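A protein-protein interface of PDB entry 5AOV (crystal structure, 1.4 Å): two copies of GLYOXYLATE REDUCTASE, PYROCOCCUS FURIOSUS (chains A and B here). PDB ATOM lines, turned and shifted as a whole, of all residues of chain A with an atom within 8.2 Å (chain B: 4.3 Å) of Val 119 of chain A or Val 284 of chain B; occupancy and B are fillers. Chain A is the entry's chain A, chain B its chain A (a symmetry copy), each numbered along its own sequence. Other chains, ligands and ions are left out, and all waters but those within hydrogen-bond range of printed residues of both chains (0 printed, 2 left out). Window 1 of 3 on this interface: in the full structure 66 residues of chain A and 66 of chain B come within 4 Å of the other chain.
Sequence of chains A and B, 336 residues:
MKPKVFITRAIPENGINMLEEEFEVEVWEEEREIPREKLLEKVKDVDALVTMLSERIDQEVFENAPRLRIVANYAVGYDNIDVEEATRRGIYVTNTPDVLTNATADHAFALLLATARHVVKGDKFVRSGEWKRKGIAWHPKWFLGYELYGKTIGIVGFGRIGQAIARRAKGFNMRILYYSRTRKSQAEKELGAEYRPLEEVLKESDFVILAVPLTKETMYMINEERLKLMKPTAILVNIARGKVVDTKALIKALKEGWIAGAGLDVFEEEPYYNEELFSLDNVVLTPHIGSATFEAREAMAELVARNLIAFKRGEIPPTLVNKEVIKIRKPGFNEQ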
ATOM      1  N   ALA A 110       5.457   6.415   4.770  1.00  0.00           N
ATOM      2  CA  ALA A 110       6.492   5.993   3.848  1.00  0.00           C
ATOM      3  C   ALA A 110       6.464   6.891   2.621  1.00  0.00           C
ATOM      4  O   ALA A 110       7.531   7.352   2.147  1.00  0.00           O
ATOM      5  CB  ALA A 110       6.308   4.538   3.469  1.00  0.00           C
ATOM      6  N   LEU A 111       5.284   7.129   2.060  1.00  0.00           N
ATOM      7  CA  LEU A 111       5.136   7.975   0.882  1.00  0.00           C
ATOM      8  C   LEU A 111       5.444   9.424   1.184  1.00  0.00           C
ATOM      9  O   LEU A 111       6.088  10.099   0.377  1.00  0.00           O
ATOM     10  CB  LEU A 111       3.737   7.839   0.284  1.00  0.00           C
ATOM     11  CG  LEU A 111       3.453   6.505  -0.344  1.00  0.00           C
ATOM     12  CD1 LEU A 111       1.990   6.482  -0.782  1.00  0.00           C
ATOM     13  CD2 LEU A 111       4.315   6.318  -1.621  1.00  0.00           C
ATOM     14  N   LEU A 112       4.997   9.948   2.301  1.00  0.00           N
ATOM     15  CA  LEU A 112       5.281  11.319   2.706  1.00  0.00           C
ATOM     16  C   LEU A 112       6.805  11.532   2.732  1.00  0.00           C
ATOM     17  O   LEU A 112       7.303  12.460   2.088  1.00  0.00           O
ATOM     18  CB  LEU A 112       4.636  11.571   4.091  1.00  0.00           C
ATOM     19  CG  LEU A 112       4.666  12.994   4.619  1.00  0.00           C
ATOM     20  CD1 LEU A 112       3.804  13.099   5.864  1.00  0.00           C
ATOM     21  CD2 LEU A 112       6.062  13.440   5.035  1.00  0.00           C
ATOM     22  N   LEU A 113       7.486  10.681   3.452  1.00  0.00           N
ATOM     23  CA  LEU A 113       8.923  10.833   3.626  1.00  0.00           C
ATOM     24  C   LEU A 113       9.704  10.577   2.351  1.00  0.00           C
ATOM     25  O   LEU A 113      10.653  11.290   2.031  1.00  0.00           O
ATOM     26  CB  LEU A 113       9.410   9.942   4.774  1.00  0.00           C
ATOM     27  CG  LEU A 113       9.009  10.421   6.165  1.00  0.00           C
ATOM     28  CD1 LEU A 113       9.134   9.333   7.172  1.00  0.00           C
ATOM     29  CD2 LEU A 113       9.867  11.652   6.550  1.00  0.00           C
ATOM     30  N   ALA A 114       9.319   9.574   1.569  1.00  0.00           N
ATOM     31  CA  ALA A 114      10.027   9.273   0.351  1.00  0.00           C
ATOM     32  C   ALA A 114       9.941  10.457  -0.586  1.00  0.00           C
ATOM     33  O   ALA A 114      10.881  10.796  -1.305  1.00  0.00           O
ATOM     34  CB  ALA A 114       9.482   8.024  -0.337  1.00  0.00           C
ATOM     35  N   THR A 115       8.752  11.072  -0.656  1.00  0.00           N
ATOM     36  CA  THR A 115       8.535  12.224  -1.556  1.00  0.00           C
ATOM     37  C   THR A 115       9.265  13.436  -1.004  1.00  0.00           C
ATOM     38  O   THR A 115       9.978  14.133  -1.766  1.00  0.00           O
ATOM     39  CB  THR A 115       7.002  12.529  -1.679  1.00  0.00           C
ATOM     40  OG1 THR A 115       6.317  11.342  -2.100  1.00  0.00           O
ATOM     41  CG2 THR A 115       6.733  13.599  -2.703  1.00  0.00           C
ATOM     42  N   ALA A 116       9.137  13.692   0.284  1.00  0.00           N
ATOM     43  CA  ALA A 116       9.768  14.875   0.851  1.00  0.00           C
ATOM     44  C   ALA A 116      11.287  14.860   0.777  1.00  0.00           C
ATOM     45  O   ALA A 116      11.886  15.952   0.706  1.00  0.00           O
ATOM     46  CB  ALA A 116       9.358  14.978   2.333  1.00  0.00           C
ATOM     47  N   ARG A 117      11.861  13.655   0.819  1.00  0.00           N
ATOM     48  CA  ARG A 117      13.340  13.527   0.921  1.00  0.00           C
ATOM     49  C   ARG A 117      13.980  12.937  -0.281  1.00  0.00           C
ATOM     50  O   ARG A 117      15.191  12.639  -0.295  1.00  0.00           O
ATOM     51  CB  ARG A 117      13.722  12.754   2.198  1.00  0.00           C
ATOM     52  CG  ARG A 117      13.178  13.483   3.467  1.00  0.00           C
ATOM     53  CD  ARG A 117      13.594  14.938   3.597  1.00  0.00           C
ATOM     54  NE  ARG A 117      15.036  15.042   3.635  1.00  0.00           N
ATOM     55  CZ  ARG A 117      15.799  14.750   4.680  1.00  0.00           C
ATOM     56  NH1 ARG A 117      15.283  14.706   5.901  1.00  0.00           N
ATOM     57  NH2 ARG A 117      17.091  14.525   4.522  1.00  0.00           N
ATOM     58  N   HIS A 118      13.232  12.759  -1.369  1.00  0.00           N
ATOM     59  CA  HIS A 118      13.823  12.326  -2.662  1.00  0.00           C
ATOM     60  C   HIS A 118      14.404  10.930  -2.602  1.00  0.00           C
ATOM     61  O   HIS A 118      15.397  10.661  -3.248  1.00  0.00           O
ATOM     62  CB  HIS A 118      14.859  13.292  -3.193  1.00  0.00           C
ATOM     63  CG  HIS A 118      14.406  14.710  -3.168  1.00  0.00           C
ATOM     64  ND1 HIS A 118      13.503  15.205  -4.085  1.00  0.00           N
ATOM     65  CD2 HIS A 118      14.807  15.754  -2.414  1.00  0.00           C
ATOM     66  CE1 HIS A 118      13.319  16.503  -3.837  1.00  0.00           C
ATOM     67  NE2 HIS A 118      14.093  16.848  -2.815  1.00  0.00           N
ATOM     68  N   VAL A 119      13.732  10.031  -1.900  1.00  0.00           N
ATOM     69  CA  VAL A 119      14.282   8.686  -1.740  1.00  0.00           C
ATOM     70  C   VAL A 119      14.342   7.886  -3.038  1.00  0.00           C
ATOM     71  O   VAL A 119      15.355   7.215  -3.298  1.00  0.00           O
ATOM     72  CB  VAL A 119      13.516   7.897  -0.634  1.00  0.00           C
ATOM     73  CG1 VAL A 119      13.936   6.415  -0.659  1.00  0.00           C
ATOM     74  CG2 VAL A 119      13.727   8.532   0.713  1.00  0.00           C
ATOM     75  N   VAL A 120      13.295   7.961  -3.845  1.00  0.00           N
ATOM     76  CA  VAL A 120      13.265   7.179  -5.121  1.00  0.00           C
ATOM     77  C   VAL A 120      14.299   7.725  -6.085  1.00  0.00           C
ATOM     78  O   VAL A 120      15.046   6.961  -6.715  1.00  0.00           O
ATOM     79  CB  VAL A 120      11.857   7.148  -5.695  1.00  0.00           C
ATOM     80  CG1 VAL A 120      11.859   6.619  -7.117  1.00  0.00           C
ATOM     81  CG2 VAL A 120      10.919   6.280  -4.773  1.00  0.00           C
ATOM     82  N   LYS A 121      14.349   9.037  -6.224  1.00  0.00           N
ATOM     83  CA  LYS A 121      15.314   9.669  -7.150  1.00  0.00           C
ATOM     84  C   LYS A 121      16.693   9.426  -6.644  1.00  0.00           C
ATOM     85  O   LYS A 121      17.649   9.171  -7.429  1.00  0.00           O
ATOM     86  CB  LYS A 121      14.996  11.184  -7.236  1.00  0.00           C
ATOM     87  CG  LYS A 121      15.938  11.944  -8.145  1.00  0.00           C
ATOM     88  CD  LYS A 121      15.395  13.282  -8.493  1.00  0.00           C
ATOM     89  CE  LYS A 121      15.742  14.305  -7.470  1.00  0.00           C
ATOM     90  NZ  LYS A 121      15.127  15.682  -7.903  1.00  0.00           N
ATOM     91  N   GLY A 122      16.971   9.535  -5.346  1.00  0.00           N
ATOM     92  CA  GLY A 122      18.240   9.276  -4.781  1.00  0.00           C
ATOM     93  C   GLY A 122      18.717   7.872  -5.004  1.00  0.00           C
ATOM     94  O   GLY A 122      19.904   7.626  -5.306  1.00  0.00           O
ATOM     95  N   ASP A 123      17.840   6.898  -4.815  1.00  0.00           N
ATOM     96  CA  ASP A 123      18.180   5.498  -4.995  1.00  0.00           C
ATOM     97  C   ASP A 123      18.566   5.289  -6.435  1.00  0.00           C
ATOM     98  O   ASP A 123      19.617   4.633  -6.697  1.00  0.00           O
ATOM     99  CB  ASP A 123      17.003   4.606  -4.588  1.00  0.00           C
ATOM    100  CG  ASP A 123      17.303   3.142  -4.725  1.00  0.00           C
ATOM    101  OD1 ASP A 123      17.347   2.659  -5.906  1.00  0.00           O
ATOM    102  OD2 ASP A 123      17.459   2.405  -3.718  1.00  0.00           O
ATOM    103  N   LYS A 124      17.832   5.790  -7.417  1.00  0.00           N
ATOM    104  CA  LYS A 124      18.168   5.601  -8.824  1.00  0.00           C
ATOM    105  C   LYS A 124      19.559   6.220  -9.110  1.00  0.00           C
ATOM    106  O   LYS A 124      20.395   5.643  -9.821  1.00  0.00           O
ATOM    107  CB  LYS A 124      17.099   6.227  -9.716  1.00  0.00           C
ATOM    108  CG  LYS A 124      17.396   6.198 -11.209  1.00  0.00           C
ATOM    109  CD  LYS A 124      16.327   6.911 -11.969  1.00  0.00           C
ATOM    110  CE  LYS A 124      16.612   6.970 -13.439  1.00  0.00           C
ATOM    111  NZ  LYS A 124      17.909   7.681 -13.627  1.00  0.00           N
ATOM    112  N   PHE A 125      19.838   7.398  -8.533  1.00  0.00           N
ATOM    113  CA  PHE A 125      21.131   8.071  -8.726  1.00  0.00           C
ATOM    114  C   PHE A 125      22.275   7.197  -8.262  1.00  0.00           C
ATOM    115  O   PHE A 125      23.315   7.107  -8.960  1.00  0.00           O
ATOM    116  CB  PHE A 125      21.083   9.464  -7.982  1.00  0.00           C
ATOM    117  CG  PHE A 125      22.323  10.317  -8.105  1.00  0.00           C
ATOM    118  CD1 PHE A 125      22.746  10.814  -9.309  1.00  0.00           C
ATOM    119  CD2 PHE A 125      23.027  10.600  -6.982  1.00  0.00           C
ATOM    120  CE1 PHE A 125      23.887  11.662  -9.388  1.00  0.00           C
ATOM    121  CE2 PHE A 125      24.100  11.467  -7.037  1.00  0.00           C
ATOM    122  CZ  PHE A 125      24.554  11.969  -8.220  1.00  0.00           C
ATOM    123  N   VAL A 126      22.136   6.588  -7.108  1.00  0.00           N
ATOM    124  CA  VAL A 126      23.183   5.715  -6.570  1.00  0.00           C
ATOM    125  C   VAL A 126      23.247   4.404  -7.386  1.00  0.00           C
ATOM    126  O   VAL A 126      24.299   3.998  -7.898  1.00  0.00           O
ATOM    127  CB  VAL A 126      22.938   5.375  -5.095  1.00  0.00           C
ATOM    128  CG1 VAL A 126      23.907   4.371  -4.585  1.00  0.00           C
ATOM    129  CG2 VAL A 126      22.996   6.663  -4.242  1.00  0.00           C
ATOM    130  N   ARG A 127      22.098   3.736  -7.487  1.00  0.00           N
ATOM    131  CA  ARG A 127      22.009   2.360  -7.983  1.00  0.00           C
ATOM    132  C   ARG A 127      22.446   2.202  -9.457  1.00  0.00           C
ATOM    133  O   ARG A 127      23.061   1.200  -9.853  1.00  0.00           O
ATOM    134  CB  ARG A 127      20.604   1.820  -7.817  1.00  0.00           C
ATOM    135  CG  ARG A 127      20.473   0.317  -7.993  1.00  0.00           C
ATOM    136  CD  ARG A 127      19.046  -0.147  -7.823  1.00  0.00           C
ATOM    137  NE  ARG A 127      18.509   0.154  -6.484  1.00  0.00           N
ATOM    138  CZ  ARG A 127      18.444  -0.756  -5.520  1.00  0.00           C
ATOM    139  NH1 ARG A 127      18.896  -1.962  -5.642  1.00  0.00           N
ATOM    140  NH2 ARG A 127      17.867  -0.351  -4.381  1.00  0.00           N
ATOM    141  N   PHE A 143      19.648  17.365  -3.594  1.00  0.00           N
ATOM    142  CA  PHE A 143      18.609  16.557  -3.000  1.00  0.00           C
ATOM    143  C   PHE A 143      17.942  17.206  -1.776  1.00  0.00           C
ATOM    144  O   PHE A 143      17.538  16.522  -0.836  1.00  0.00           O
ATOM    145  CB  PHE A 143      19.123  15.149  -2.609  1.00  0.00           C
ATOM    146  CG  PHE A 143      19.536  14.293  -3.821  1.00  0.00           C
ATOM    147  CD1 PHE A 143      18.565  13.771  -4.622  1.00  0.00           C
ATOM    148  CD2 PHE A 143      20.835  14.081  -4.099  1.00  0.00           C
ATOM    149  CE1 PHE A 143      18.932  12.998  -5.760  1.00  0.00           C
ATOM    150  CE2 PHE A 143      21.226  13.326  -5.221  1.00  0.00           C
ATOM    151  CZ  PHE A 143      20.283  12.800  -6.010  1.00  0.00           C
ATOM    152  N   ASP A 281       9.992  13.673 -11.603  1.00  0.00           N
ATOM    153  CA  ASP A 281      10.800  13.168 -10.507  1.00  0.00           C
ATOM    154  C   ASP A 281      10.305  13.637  -9.156  1.00  0.00           C
ATOM    155  O   ASP A 281      10.868  13.153  -8.175  1.00  0.00           O
ATOM    156  CB  ASP A 281      12.264  13.522 -10.649  1.00  0.00           C
ATOM    157  CG  ASP A 281      12.478  14.981 -10.760  1.00  0.00           C
ATOM    158  OD1 ASP A 281      11.664  15.814 -10.321  1.00  0.00           O
ATOM    159  OD2 ASP A 281      13.541  15.329 -11.368  1.00  0.00           O
ATOM    160  N   VAL A 284       6.240  10.114  -6.222  1.00  0.00           N
ATOM    161  CA  VAL A 284       6.558   8.753  -5.774  1.00  0.00           C
ATOM    162  C   VAL A 284       5.315   7.901  -5.940  1.00  0.00           C
ATOM    163  O   VAL A 284       4.195   8.382  -5.593  1.00  0.00           O
ATOM    164  CB  VAL A 284       7.061   8.732  -4.333  1.00  0.00           C
ATOM    165  CG1 VAL A 284       7.231   7.268  -3.821  1.00  0.00           C
ATOM    166  CG2 VAL A 284       8.396   9.487  -4.227  1.00  0.00           C
ATOM    167  N   HIS B 107      15.126  11.255   7.864  1.00  0.00           N
ATOM    168  CA  HIS B 107      15.652  10.427   6.781  1.00  0.00           C
ATOM    169  C   HIS B 107      15.854   9.016   7.244  1.00  0.00           C
ATOM    170  O   HIS B 107      15.640   8.051   6.458  1.00  0.00           O
ATOM    171  CB  HIS B 107      16.973  10.992   6.276  1.00  0.00           C
ATOM    172  CG  HIS B 107      17.276  10.463   4.897  1.00  0.00           C
ATOM    173  ND1 HIS B 107      16.463  10.755   3.817  1.00  0.00           N
ATOM    174  CD2 HIS B 107      18.259   9.638   4.453  1.00  0.00           C
ATOM    175  CE1 HIS B 107      16.977  10.133   2.744  1.00  0.00           C
ATOM    176  NE2 HIS B 107      18.032   9.425   3.132  1.00  0.00           N
ATOM    177  N   ALA B 110      12.571   7.650   6.784  1.00  0.00           N
ATOM    178  CA  ALA B 110      12.295   7.509   5.368  1.00  0.00           C
ATOM    179  C   ALA B 110      12.883   6.197   4.872  1.00  0.00           C
ATOM    180  O   ALA B 110      12.212   5.443   4.126  1.00  0.00           O
ATOM    181  CB  ALA B 110      12.853   8.688   4.597  1.00  0.00           C
ATOM    182  N   LEU B 111      14.131   5.910   5.226  1.00  0.00           N
ATOM    183  CA  LEU B 111      14.796   4.681   4.810  1.00  0.00           C
ATOM    184  C   LEU B 111      14.181   3.459   5.454  1.00  0.00           C
ATOM    185  O   LEU B 111      14.014   2.431   4.793  1.00  0.00           O
ATOM    186  CB  LEU B 111      16.293   4.744   5.106  1.00  0.00           C
ATOM    187  CG  LEU B 111      17.056   5.724   4.261  1.00  0.00           C
ATOM    188  CD1 LEU B 111      18.501   5.760   4.754  1.00  0.00           C
ATOM    189  CD2 LEU B 111      17.088   5.249   2.783  1.00  0.00           C
ATOM    190  N   ALA B 114      10.774   2.963   3.630  1.00  0.00           N
ATOM    191  CA  ALA B 114      10.915   2.636   2.234  1.00  0.00           C
ATOM    192  C   ALA B 114      11.349   1.194   2.097  1.00  0.00           C
ATOM    193  O   ALA B 114      10.935   0.466   1.195  1.00  0.00           O
ATOM    194  CB  ALA B 114      11.913   3.550   1.527  1.00  0.00           C
ATOM    195  N   THR B 115      12.279   0.770   2.964  1.00  0.00           N
ATOM    196  CA  THR B 115      12.805  -0.609   2.914  1.00  0.00           C
ATOM    197  C   THR B 115      11.735  -1.572   3.405  1.00  0.00           C
ATOM    198  O   THR B 115      11.484  -2.609   2.746  1.00  0.00           O
ATOM    199  CB  THR B 115      14.087  -0.730   3.807  1.00  0.00           C
ATOM    200  OG1 THR B 115      15.042   0.258   3.397  1.00  0.00           O
ATOM    201  CG2 THR B 115      14.736  -2.080   3.663  1.00  0.00           C
ATOM    202  N   VAL B 120      10.758   1.645  -3.152  1.00  0.00           N
ATOM    203  CA  VAL B 120      11.600   1.827  -4.376  1.00  0.00           C
ATOM    204  C   VAL B 120      11.218   0.798  -5.421  1.00  0.00           C
ATOM    205  O   VAL B 120      11.061   1.125  -6.607  1.00  0.00           O
ATOM    206  CB  VAL B 120      13.077   1.807  -4.016  1.00  0.00           C
ATOM    207  CG1 VAL B 120      13.941   1.695  -5.258  1.00  0.00           C
ATOM    208  CG2 VAL B 120      13.447   3.095  -3.187  1.00  0.00           C
ATOM    209  N   ALA B 262      17.825  -3.738   4.059  1.00  0.00           N
ATOM    210  CA  ALA B 262      18.624  -2.650   4.598  1.00  0.00           C
ATOM    211  C   ALA B 262      18.388  -1.376   3.847  1.00  0.00           C
ATOM    212  O   ALA B 262      18.251  -1.394   2.599  1.00  0.00           O
ATOM    213  CB  ALA B 262      20.144  -2.959   4.512  1.00  0.00           C
ATOM    214  N   GLY B 263      18.356  -0.273   4.571  1.00  0.00           N
ATOM    215  CA  GLY B 263      18.301   1.084   4.012  1.00  0.00           C
ATOM    216  C   GLY B 263      19.569   1.822   4.337  1.00  0.00           C
ATOM    217  O   GLY B 263      19.913   1.923   5.545  1.00  0.00           O
ATOM    218  N   LEU B 264      20.309   2.286   3.362  1.00  0.00           N
ATOM    219  CA  LEU B 264      21.656   2.791   3.569  1.00  0.00           C
ATOM    220  C   LEU B 264      21.800   4.168   2.979  1.00  0.00           C
ATOM    221  O   LEU B 264      21.534   4.351   1.782  1.00  0.00           O
ATOM    222  CB  LEU B 264      22.674   1.887   2.886  1.00  0.00           C
ATOM    223  CG  LEU B 264      22.597   0.392   3.254  1.00  0.00           C
ATOM    224  CD1 LEU B 264      23.574  -0.387   2.327  1.00  0.00           C
ATOM    225  CD2 LEU B 264      22.915   0.103   4.701  1.00  0.00           C
ATOM    226  N   VAL B 283      17.419  -3.796  -0.729  1.00  0.00           N
ATOM    227  CA  VAL B 283      18.149  -2.647  -0.218  1.00  0.00           C
ATOM    228  C   VAL B 283      17.529  -1.385  -0.821  1.00  0.00           C
ATOM    229  O   VAL B 283      17.046  -1.402  -1.955  1.00  0.00           O
ATOM    230  CB  VAL B 283      19.701  -2.762  -0.518  1.00  0.00           C
ATOM    231  CG1 VAL B 283      20.049  -2.502  -1.984  1.00  0.00           C
ATOM    232  CG2 VAL B 283      20.502  -1.869   0.355  1.00  0.00           C
ATOM    233  N   VAL B 284      17.572  -0.329  -0.033  1.00  0.00           N
ATOM    234  CA  VAL B 284      17.244   1.040  -0.450  1.00  0.00           C
ATOM    235  C   VAL B 284      18.469   1.905  -0.227  1.00  0.00           C
ATOM    236  O   VAL B 284      19.127   1.765   0.847  1.00  0.00           O
ATOM    237  CB  VAL B 284      16.030   1.586   0.297  1.00  0.00           C
ATOM    238  CG1 VAL B 284      15.802   3.094  -0.035  1.00  0.00           C
ATOM    239  CG2 VAL B 284      14.777   0.771  -0.061  1.00  0.00           C
ATOM    240  N   LEU B 285      18.811   2.744  -1.178  1.00  0.00           N
ATOM    241  CA  LEU B 285      20.074   3.475  -1.185  1.00  0.00           C
ATOM    242  C   LEU B 285      19.841   4.949  -1.357  1.00  0.00           C
ATOM    243  O   LEU B 285      19.008   5.338  -2.184  1.00  0.00           O
ATOM    244  CB  LEU B 285      20.872   3.001  -2.410  1.00  0.00           C
ATOM    245  CG  LEU B 285      21.081   1.490  -2.520  1.00  0.00           C
ATOM    246  CD1 LEU B 285      21.470   1.109  -3.988  1.00  0.00           C
ATOM    247  CD2 LEU B 285      22.215   1.073  -1.588  1.00  0.00           C
ATOM    248  N   THR B 286      20.526   5.785  -0.580  1.00  0.00           N
ATOM    249  CA  THR B 286      20.510   7.232  -0.829  1.00  0.00           C
ATOM    250  C   THR B 286      21.925   7.798  -0.691  1.00  0.00           C
ATOM    251  O   THR B 286      22.735   7.232   0.083  1.00  0.00           O
ATOM    252  CB  THR B 286      19.498   8.033   0.055  1.00  0.00           C
ATOM    253  OG1 THR B 286      19.709   7.744   1.415  1.00  0.00           O
ATOM    254  CG2 THR B 286      18.081   7.642  -0.219  1.00  0.00           C
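Of the printed residues of chain B, Leu 113 of chain A touches Ala 110 (3.7 Å). Of the printed residues of chain B, Val 119 of chain A touches Ala 110 (3.98 Å) and Val 284 (3.9 Å). Of the printed residues of chain B, Arg 127 of chain A touches Val 283 and Leu 285. Leu 111 of chain B touches none of the printed residues of chain A. Of the printed residues of chain A, Val 120 of chain B touches Asp 123. Ala 262 of chain B touches none of the printed residues of chain A. Printed residues of chain A within 4 Å of Val 284 of chain B: Val 119 and Asp 123. The nearest printed residue of chain B that does not touch Val 119 of chain A is Ala 114 of chain B (4.1 Å).
Of the 13 printed residues of chain B, 7 touch a printed residue of chain A. Along chain B the printed residues that touch a printed residue of chain A span positions 107 to 286. Hydrophobic or aromatic side chains of chain A within 4 Å of the printed part of chain B: Leu 113, Val 119 and Val 126. Among the printed residues, 12 pairs touch across the chains. Among the printed residues, no Asp or Glu carboxylate lies within 4 Å of a Lys or Arg side-chain nitrogen of the other chain.
Ala 110 of chain B touches Leu 113 of chain A. Arg 117 of chain A touches His 107 of chain B. CB of Ala 110 of chain B touches CG2 of Val 119 of chain A (3.98 Å). Val 284 of chain B touches Val 119 of chain A. Leu 285 of chain B touches Gly 122 of chain A (O to C, 3.8 Å). OD1 of Asp 123 of chain A touches CG1 of Val 120 of chain B (3.6 Å). Val 284 of chain B touches Asp 123 of chain A. Leu 285 of chain B touches Val 126 of chain A. Thr 286 of chain B touches Val 126 of chain A. CD1 of Leu 285 of chain B touches CZ of Arg 127 of chain A (3.9 Å).
The side-chain carboxylate (OD2) of Asp 123 of chain A lies within hydrogen-bond range of the backbone NH (N) of Leu 285 of chain B, at 2.9 Å. NH2 of Arg 127 of chain A is in hydrogen-bond range of O of Val 283 of chain B, 2.8 Å away.
The backbone NH of Thr 286 of chain B is in hydrogen-bond range of the backbone carbonyl oxygen of Leu 264 of chain B (2.9 Å). A ring nitrogen (NE2) of His 107 of chain B lies within hydrogen-bond range of the side-chain hydroxyl (OG1) of Thr 286 of chain B (2.9 Å). The guanidinium group (NE) of Arg 127 of chain A is in salt-bridge range of the side-chain carboxylate (OD1) of Asp 123 of chain A, 2.8 Å away. The backbone NH (N) of Val 119 of chain A lies within hydrogen-bond range of the backbone carbonyl oxygen (O) of Ala 114 of chain A (3.0 Å). The backbone carbonyl oxygen of Val 284 of chain B lies within hydrogen-bond range of the backbone NH of Leu 264 of chain B, at 2.8 Å. O of Ala 262 of chain B sits at hydrogen-bond distance from N of Val 284 of chain B, 2.9 Å away.
Positions printed for both chains: 110, 111, 114, 115, 120 and 284.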
